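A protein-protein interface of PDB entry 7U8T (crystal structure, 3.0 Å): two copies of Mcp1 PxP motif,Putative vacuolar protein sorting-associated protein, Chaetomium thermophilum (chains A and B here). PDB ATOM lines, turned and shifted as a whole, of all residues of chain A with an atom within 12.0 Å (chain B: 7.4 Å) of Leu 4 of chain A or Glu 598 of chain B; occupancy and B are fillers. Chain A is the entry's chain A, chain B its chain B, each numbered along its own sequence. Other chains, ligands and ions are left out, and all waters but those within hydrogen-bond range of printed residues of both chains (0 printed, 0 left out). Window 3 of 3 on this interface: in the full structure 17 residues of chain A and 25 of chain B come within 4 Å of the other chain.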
ATOM      1  N   SER A   3      23.589  -2.513 -17.486  1.00  0.00           N
ATOM      2  CA  SER A   3      23.493  -1.071 -17.284  1.00  0.00           C
ATOM      3  C   SER A   3      22.066  -0.662 -16.944  1.00  0.00           C
ATOM      4  O   SER A   3      21.211  -1.512 -16.682  1.00  0.00           O
ATOM      5  CB  SER A   3      23.971  -0.320 -18.530  1.00  0.00           C
ATOM      6  OG  SER A   3      23.128  -0.583 -19.641  1.00  0.00           O
ATOM      7  N   LEU A   4      21.814   0.646 -16.945  1.00  0.00           N
ATOM      8  CA  LEU A   4      20.492   1.192 -16.679  1.00  0.00           C
ATOM      9  C   LEU A   4      19.963   1.908 -17.916  1.00  0.00           C
ATOM     10  O   LEU A   4      20.727   2.373 -18.768  1.00  0.00           O
ATOM     11  CB  LEU A   4      20.503   2.155 -15.481  1.00  0.00           C
ATOM     12  CG  LEU A   4      21.038   1.657 -14.132  1.00  0.00           C
ATOM     13  CD1 LEU A   4      20.622   2.619 -13.037  1.00  0.00           C
ATOM     14  CD2 LEU A   4      20.573   0.239 -13.796  1.00  0.00           C
ATOM     15  N   VAL A   5      18.637   1.993 -18.001  1.00  0.00           N
ATOM     16  CA  VAL A   5      17.969   2.540 -19.176  1.00  0.00           C
ATOM     17  C   VAL A   5      17.978   4.060 -19.085  1.00  0.00           C
ATOM     18  O   VAL A   5      17.382   4.642 -18.173  1.00  0.00           O
ATOM     19  CB  VAL A   5      16.536   2.004 -19.299  1.00  0.00           C
ATOM     20  CG1 VAL A   5      15.827   2.639 -20.485  1.00  0.00           C
ATOM     21  CG2 VAL A   5      16.551   0.487 -19.430  1.00  0.00           C
ATOM     22  N   GLU A   6      18.650   4.704 -20.034  1.00  0.00           N
ATOM     23  CA  GLU A   6      18.774   6.155 -20.033  1.00  0.00           C
ATOM     24  C   GLU A   6      17.505   6.784 -20.593  1.00  0.00           C
ATOM     25  O   GLU A   6      17.056   6.427 -21.687  1.00  0.00           O
ATOM     26  CB  GLU A   6      19.991   6.576 -20.853  1.00  0.00           C
ATOM     27  CG  GLU A   6      21.307   6.112 -20.258  1.00  0.00           C
ATOM     28  CD  GLU A   6      22.493   6.484 -21.117  1.00  0.00           C
ATOM     29  OE1 GLU A   6      22.274   6.946 -22.257  1.00  0.00           O
ATOM     30  OE2 GLU A   6      23.642   6.305 -20.658  1.00  0.00           O
ATOM     31  N   LEU A   7      16.925   7.715 -19.839  1.00  0.00           N
ATOM     32  CA  LEU A   7      15.685   8.371 -20.225  1.00  0.00           C
ATOM     33  C   LEU A   7      15.904   9.858 -20.442  1.00  0.00           C
ATOM     34  O   LEU A   7      16.793  10.472 -19.845  1.00  0.00           O
ATOM     35  CB  LEU A   7      14.601   8.183 -19.174  1.00  0.00           C
ATOM     36  CG  LEU A   7      14.494   6.793 -18.564  1.00  0.00           C
ATOM     37  CD1 LEU A   7      13.550   6.863 -17.409  1.00  0.00           C
ATOM     38  CD2 LEU A   7      13.988   5.814 -19.601  1.00  0.00           C
ATOM     39  N   ASP A   8      15.075  10.428 -21.308  1.00  0.00           N
ATOM     40  CA  ASP A   8      15.055  11.866 -21.485  1.00  0.00           C
ATOM     41  C   ASP A   8      14.368  12.513 -20.281  1.00  0.00           C
ATOM     42  O   ASP A   8      13.486  11.909 -19.664  1.00  0.00           O
ATOM     43  CB  ASP A   8      14.334  12.228 -22.783  1.00  0.00           C
ATOM     44  CG  ASP A   8      15.250  12.153 -23.998  1.00  0.00           C
ATOM     45  OD1 ASP A   8      16.447  12.499 -23.873  1.00  0.00           O
ATOM     46  OD2 ASP A   8      14.771  11.748 -25.080  1.00  0.00           O
ATOM     47  N   MET B 595      19.165  11.295 -11.438  1.00  0.00           N
ATOM     48  CA  MET B 595      18.357  10.349 -10.677  1.00  0.00           C
ATOM     49  C   MET B 595      18.628   8.948 -11.205  1.00  0.00           C
ATOM     50  O   MET B 595      18.300   8.635 -12.354  1.00  0.00           O
ATOM     51  CB  MET B 595      16.881  10.708 -10.797  1.00  0.00           C
ATOM     52  CG  MET B 595      16.612  12.156 -10.466  1.00  0.00           C
ATOM     53  SD  MET B 595      17.111  12.536  -8.783  1.00  0.00           S
ATOM     54  CE  MET B 595      16.768  14.280  -8.726  1.00  0.00           C
ATOM     55  N   ARG B 596      19.220   8.109 -10.363  1.00  0.00           N
ATOM     56  CA  ARG B 596      19.684   6.778 -10.740  1.00  0.00           C
ATOM     57  C   ARG B 596      18.911   5.765  -9.894  1.00  0.00           C
ATOM     58  O   ARG B 596      19.199   5.586  -8.706  1.00  0.00           O
ATOM     59  CB  ARG B 596      21.200   6.680 -10.545  1.00  0.00           C
ATOM     60  CG  ARG B 596      21.801   5.301 -10.716  1.00  0.00           C
ATOM     61  CD  ARG B 596      23.324   5.332 -10.626  1.00  0.00           C
ATOM     62  NE  ARG B 596      23.917   4.091 -11.114  1.00  0.00           N
ATOM     63  CZ  ARG B 596      24.105   3.792 -12.394  1.00  0.00           C
ATOM     64  NH1 ARG B 596      23.840   4.661 -13.356  1.00  0.00           N
ATOM     65  NH2 ARG B 596      24.575   2.589 -12.715  1.00  0.00           N
ATOM     66  N   ASN B 597      17.909   5.120 -10.490  1.00  0.00           N
ATOM     67  CA  ASN B 597      17.104   4.110  -9.806  1.00  0.00           C
ATOM     68  C   ASN B 597      17.688   2.742 -10.141  1.00  0.00           C
ATOM     69  O   ASN B 597      17.414   2.178 -11.206  1.00  0.00           O
ATOM     70  CB  ASN B 597      15.641   4.211 -10.220  1.00  0.00           C
ATOM     71  CG  ASN B 597      14.729   3.315  -9.392  1.00  0.00           C
ATOM     72  OD1 ASN B 597      15.125   2.778  -8.356  1.00  0.00           O
ATOM     73  ND2 ASN B 597      13.493   3.154  -9.850  1.00  0.00           N
ATOM     74  N   GLU B 598      18.492   2.215  -9.222  1.00  0.00           N
ATOM     75  CA  GLU B 598      19.080   0.888  -9.342  1.00  0.00           C
ATOM     76  C   GLU B 598      18.195  -0.201  -8.751  1.00  0.00           C
ATOM     77  O   GLU B 598      18.583  -1.376  -8.776  1.00  0.00           O
ATOM     78  CB  GLU B 598      20.452   0.855  -8.656  1.00  0.00           C
ATOM     79  CG  GLU B 598      21.487   1.802  -9.247  1.00  0.00           C
ATOM     80  CD  GLU B 598      22.867   1.609  -8.637  1.00  0.00           C
ATOM     81  OE1 GLU B 598      22.951   1.130  -7.485  1.00  0.00           O
ATOM     82  OE2 GLU B 598      23.866   1.933  -9.313  1.00  0.00           O
ATOM     83  N   SER B 599      17.028   0.156  -8.220  1.00  0.00           N
ATOM     84  CA  SER B 599      16.144  -0.790  -7.560  1.00  0.00           C
ATOM     85  C   SER B 599      15.092  -1.321  -8.532  1.00  0.00           C
ATOM     86  O   SER B 599      14.965  -0.861  -9.668  1.00  0.00           O
ATOM     87  CB  SER B 599      15.463  -0.135  -6.358  1.00  0.00           C
ATOM     88  OG  SER B 599      14.609   0.917  -6.773  1.00  0.00           O
ATOM     89  N   ASP B 600      14.315  -2.297  -8.060  1.00  0.00           N
ATOM     90  CA  ASP B 600      13.248  -2.904  -8.847  1.00  0.00           C
ATOM     91  C   ASP B 600      11.884  -2.269  -8.580  1.00  0.00           C
ATOM     92  O   ASP B 600      10.859  -2.957  -8.637  1.00  0.00           O
ATOM     93  CB  ASP B 600      13.194  -4.415  -8.598  1.00  0.00           C
ATOM     94  CG  ASP B 600      13.046  -4.774  -7.119  1.00  0.00           C
ATOM     95  OD1 ASP B 600      13.145  -3.875  -6.251  1.00  0.00           O
ATOM     96  OD2 ASP B 600      12.823  -5.968  -6.825  1.00  0.00           O
ATOM     97  N   THR B 601      11.849  -0.968  -8.296  1.00  0.00           N
ATOM     98  CA  THR B 601      10.630  -0.286  -7.883  1.00  0.00           C
ATOM     99  C   THR B 601      10.477   1.015  -8.659  1.00  0.00           C
ATOM    100  O   THR B 601      11.394   1.843  -8.674  1.00  0.00           O
ATOM    101  CB  THR B 601      10.650  -0.001  -6.376  1.00  0.00           C
ATOM    102  OG1 THR B 601      11.040  -1.184  -5.670  1.00  0.00           O
ATOM    103  CG2 THR B 601       9.283   0.436  -5.897  1.00  0.00           C
ATOM    104  N   LEU B 630      10.179   7.599 -12.630  1.00  0.00           N
ATOM    105  CA  LEU B 630      11.483   6.948 -12.633  1.00  0.00           C
ATOM    106  C   LEU B 630      11.240   5.444 -12.564  1.00  0.00           C
ATOM    107  O   LEU B 630      11.098   4.884 -11.466  1.00  0.00           O
ATOM    108  CB  LEU B 630      12.333   7.449 -11.468  1.00  0.00           C
ATOM    109  CG  LEU B 630      13.841   7.237 -11.557  1.00  0.00           C
ATOM    110  CD1 LEU B 630      14.388   7.920 -12.794  1.00  0.00           C
ATOM    111  CD2 LEU B 630      14.514   7.781 -10.306  1.00  0.00           C
ATOM    112  N   PRO B 631      11.175   4.758 -13.709  1.00  0.00           N
ATOM    113  CA  PRO B 631      10.925   3.291 -13.736  1.00  0.00           C
ATOM    114  C   PRO B 631      12.092   2.501 -13.156  1.00  0.00           C
ATOM    115  O   PRO B 631      13.174   3.071 -12.951  1.00  0.00           O
ATOM    116  CB  PRO B 631      10.741   3.012 -15.243  1.00  0.00           C
ATOM    117  CG  PRO B 631      11.399   4.143 -15.934  1.00  0.00           C
ATOM    118  CD  PRO B 631      11.151   5.332 -15.062  1.00  0.00           C
ATOM    119  N   PRO B 632      11.906   1.202 -12.837  1.00  0.00           N
ATOM    120  CA  PRO B 632      13.013   0.424 -12.249  1.00  0.00           C
ATOM    121  C   PRO B 632      14.188   0.221 -13.196  1.00  0.00           C
ATOM    122  O   PRO B 632      14.006  -0.024 -14.393  1.00  0.00           O
ATOM    123  CB  PRO B 632      12.359  -0.922 -11.907  1.00  0.00           C
ATOM    124  CG  PRO B 632      10.940  -0.629 -11.759  1.00  0.00           C
ATOM    125  CD  PRO B 632      10.636   0.451 -12.737  1.00  0.00           C
ATOM    126  N   ARG B 633      15.393   0.327 -12.615  1.00  0.00           N
ATOM    127  CA  ARG B 633      16.694   0.242 -13.293  1.00  0.00           C
ATOM    128  C   ARG B 633      16.801   1.272 -14.421  1.00  0.00           C
ATOM    129  O   ARG B 633      16.959   0.938 -15.596  1.00  0.00           O
ATOM    130  CB  ARG B 633      16.970  -1.185 -13.794  1.00  0.00           C
ATOM    131  N   SER B 634      16.709   2.545 -14.040  1.00  0.00           N
ATOM    132  CA  SER B 634      16.712   3.631 -15.011  1.00  0.00           C
ATOM    133  C   SER B 634      17.552   4.789 -14.487  1.00  0.00           C
ATOM    134  O   SER B 634      17.980   4.804 -13.332  1.00  0.00           O
ATOM    135  CB  SER B 634      15.289   4.108 -15.325  1.00  0.00           C
ATOM    136  OG  SER B 634      14.771   4.878 -14.255  1.00  0.00           O
ATOM    137  N   ILE B 635      17.789   5.768 -15.355  1.00  0.00           N
ATOM    138  CA  ILE B 635      18.557   6.954 -14.987  1.00  0.00           C
ATOM    139  C   ILE B 635      18.023   8.129 -15.802  1.00  0.00           C
ATOM    140  O   ILE B 635      17.650   7.980 -16.970  1.00  0.00           O
ATOM    141  CB  ILE B 635      20.080   6.707 -15.164  1.00  0.00           C
ATOM    142  CG1 ILE B 635      20.913   7.889 -14.657  1.00  0.00           C
ATOM    143  CG2 ILE B 635      20.448   6.322 -16.598  1.00  0.00           C
ATOM    144  CD1 ILE B 635      22.383   7.573 -14.523  1.00  0.00           C
ATOM    145  N   ILE B 684      14.152   0.352   0.402  1.00  0.00           N
ATOM    146  CA  ILE B 684      14.938   1.069  -0.598  1.00  0.00           C
ATOM    147  C   ILE B 684      15.989   1.912   0.111  1.00  0.00           C
ATOM    148  O   ILE B 684      15.654   2.809   0.897  1.00  0.00           O
ATOM    149  CB  ILE B 684      14.046   1.947  -1.489  1.00  0.00           C
ATOM    150  CG1 ILE B 684      12.973   1.098  -2.177  1.00  0.00           C
ATOM    151  CG2 ILE B 684      14.888   2.692  -2.516  1.00  0.00           C
ATOM    152  CD1 ILE B 684      13.528   0.002  -3.051  1.00  0.00           C
ATOM    153  N   LEU B 697      21.672  10.827  -7.315  1.00  0.00           N
ATOM    154  CA  LEU B 697      20.812  10.166  -6.340  1.00  0.00           C
ATOM    155  C   LEU B 697      20.668   8.695  -6.719  1.00  0.00           C
ATOM    156  O   LEU B 697      20.186   8.378  -7.811  1.00  0.00           O
ATOM    157  CB  LEU B 697      19.439  10.835  -6.289  1.00  0.00           C
ATOM    158  CG  LEU B 697      18.398  10.148  -5.400  1.00  0.00           C
ATOM    159  CD1 LEU B 697      18.883  10.118  -3.967  1.00  0.00           C
ATOM    160  CD2 LEU B 697      17.040  10.818  -5.488  1.00  0.00           C
ATOM    161  N   ILE B 698      21.069   7.800  -5.820  1.00  0.00           N
ATOM    162  CA  ILE B 698      21.070   6.365  -6.073  1.00  0.00           C
ATOM    163  C   ILE B 698      20.047   5.714  -5.153  1.00  0.00           C
ATOM    164  O   ILE B 698      20.170   5.788  -3.922  1.00  0.00           O
ATOM    165  CB  ILE B 698      22.465   5.753  -5.870  1.00  0.00           C
ATOM    166  CG1 ILE B 698      23.441   6.276  -6.929  1.00  0.00           C
ATOM    167  CG2 ILE B 698      22.386   4.229  -5.923  1.00  0.00           C
ATOM    168  CD1 ILE B 698      24.888   5.905  -6.669  1.00  0.00           C
ATOM    169  N   LEU B 699      19.035   5.080  -5.756  1.00  0.00           N
ATOM    170  CA  LEU B 699      18.019   4.302  -5.050  1.00  0.00           C
ATOM    171  C   LEU B 699      18.275   2.827  -5.332  1.00  0.00           C
ATOM    172  O   LEU B 699      18.139   2.380  -6.475  1.00  0.00           O
ATOM    173  CB  LEU B 699      16.612   4.694  -5.496  1.00  0.00           C
ATOM    174  CG  LEU B 699      16.170   6.151  -5.370  1.00  0.00           C
ATOM    175  CD1 LEU B 699      14.730   6.296  -5.837  1.00  0.00           C
ATOM    176  CD2 LEU B 699      16.328   6.642  -3.943  1.00  0.00           C
ATOM    177  N   SER B 700      18.627   2.070  -4.296  1.00  0.00           N
ATOM    178  CA  SER B 700      19.004   0.672  -4.456  1.00  0.00           C
ATOM    179  C   SER B 700      18.145  -0.215  -3.564  1.00  0.00           C
ATOM    180  O   SER B 700      17.402   0.261  -2.704  1.00  0.00           O
ATOM    181  CB  SER B 700      20.491   0.462  -4.137  1.00  0.00           C
ATOM    182  OG  SER B 700      20.797   0.868  -2.813  1.00  0.00           O
ATOM    183  N   ASN B 701      18.262  -1.524  -3.777  1.00  0.00           N
ATOM    184  CA  ASN B 701      17.559  -2.508  -2.966  1.00  0.00           C
ATOM    185  C   ASN B 701      18.405  -2.900  -1.760  1.00  0.00           C
ATOM    186  O   ASN B 701      19.620  -3.090  -1.873  1.00  0.00           O
ATOM    187  CB  ASN B 701      17.230  -3.757  -3.787  1.00  0.00           C
ATOM    188  CG  ASN B 701      16.070  -3.544  -4.738  1.00  0.00           C
ATOM    189  OD1 ASN B 701      16.191  -3.766  -5.942  1.00  0.00           O
ATOM    190  ND2 ASN B 701      14.937  -3.110  -4.199  1.00  0.00           N
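Among the printed residues, merely in contact across the chains: Leu 4 of chain A with Arg 596 of chain B (3.7 Å), Leu 4 of chain A with Asn 597 of chain B (3.7 Å), Leu 4 of chain A with Glu 598 of chain B (3.97 Å), Leu 4 of chain A with Arg 633 of chain B (3.7 Å), Leu 4 of chain A with Ser 634 of chain B (3.4 Å), Val 5 of chain A with Ser 634 of chain B (3.4 Å), Glu 6 of chain A with Ile 635 of chain B (3.7 Å), Leu 7 of chain A with Pro 631 of chain B (3.7 Å) and Leu 7 of chain A with Ser 634 of chain B (3.9 Å).
Of chain B, only Arg 596, Asn 597, Glu 598, Arg 633 and Ser 634 come within 4 Å of Leu 4 of chain A. Of chain A, only Leu 4 comes within 4 Å of Glu 598 of chain B. No residue of chain A comes within 4 Å of Asp 600 of chain B. Arg 633 of chain B touches just these residues of chain A: Leu 4 and Val 5. Of the printed residues of chain A, Ser 634 of chain B touches Leu 4, Val 5 and Leu 7. Ile 635 of chain B touches just these residues of chain A: Val 5 (3.1 Å), Glu 6 (3.7 Å) and Leu 7 (3.0 Å). Ile 698 of chain B touches none of the printed residues of chain A. No residue of chain A comes within 4 Å of Ser 700 of chain B. No residue of chain A comes within 4 Å of Asn 701 of chain B. Printed residues of chain B within 4 Å of Leu 7 of chain A: Pro 631 (3.7 Å), Ser 634 (3.9 Å) and Ile 635 (3.0 Å). Of the printed residues of chain B, Glu 6 of chain A touches Ile 635 (3.7 Å). Of the printed residues of chain A, Pro 631 of chain B touches Leu 7. Ile 684 of chain B touches none of the printed residues of chain A. Leu 630 of chain B touches none of the printed residues of chain A. The nearest residue of chain B that does not touch Leu 4 of chain A is Ile 635 of chain B (4.3 Å). The nearest residue of chain A that does not touch Glu 598 of chain B is Ser 3 of chain A (8.0 Å).
OE2 of Glu 598 of chain B lies within salt-bridge range of NE of Arg 596 of chain B (2.8 Å). The backbone NH (N) of Arg 596 of chain B sits at hydrogen-bond distance from the backbone carbonyl oxygen (O) of Leu 697 of chain B, 2.7 Å away. The backbone NH (N) of Leu 699 of chain B lies within hydrogen-bond range of the backbone carbonyl oxygen (O) of Arg 596 of chain B (3.0 Å). The side-chain hydroxyl of Ser 599 of chain B sits at hydrogen-bond distance from the side-chain amide oxygen of Asn 597 of chain B, 2.5 Å away. The backbone NH of Asn 597 of chain B lies within hydrogen-bond range of the backbone carbonyl oxygen of Ser 634 of chain B (2.9 Å). The backbone carbonyl oxygen (O) of Pro 631 of chain B sits at hydrogen-bond distance from the side-chain hydroxyl (OG) of Ser 634 of chain B.
No position is printed for both chains. Of the 12 pairs that touch across the chains among the printed residues, none has its exchanged pair printed and touching as well.
The backbone NH of Val 5 of chain A sits at hydrogen-bond distance from the backbone carbonyl oxygen of Arg 633 of chain B. The backbone carbonyl oxygen of Val 5 of chain A lies within hydrogen-bond range of the backbone NH of Ile 635 of chain B. The backbone carbonyl oxygen (O) of Ile 635 of chain B lies within hydrogen-bond range of the backbone NH (N) of Leu 7 of chain A (3.0 Å).
Of the 6 printed residues of chain A, 4 touch a printed residue of chain B. Hydrophobic or aromatic side chains of chain A within 4 Å of the printed part of chain B: Leu 4, Val 5 and Leu 7. Among the printed residues, no Asp or Glu carboxylate lies within 4 Å of a Lys or Arg side-chain nitrogen of the other chain.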
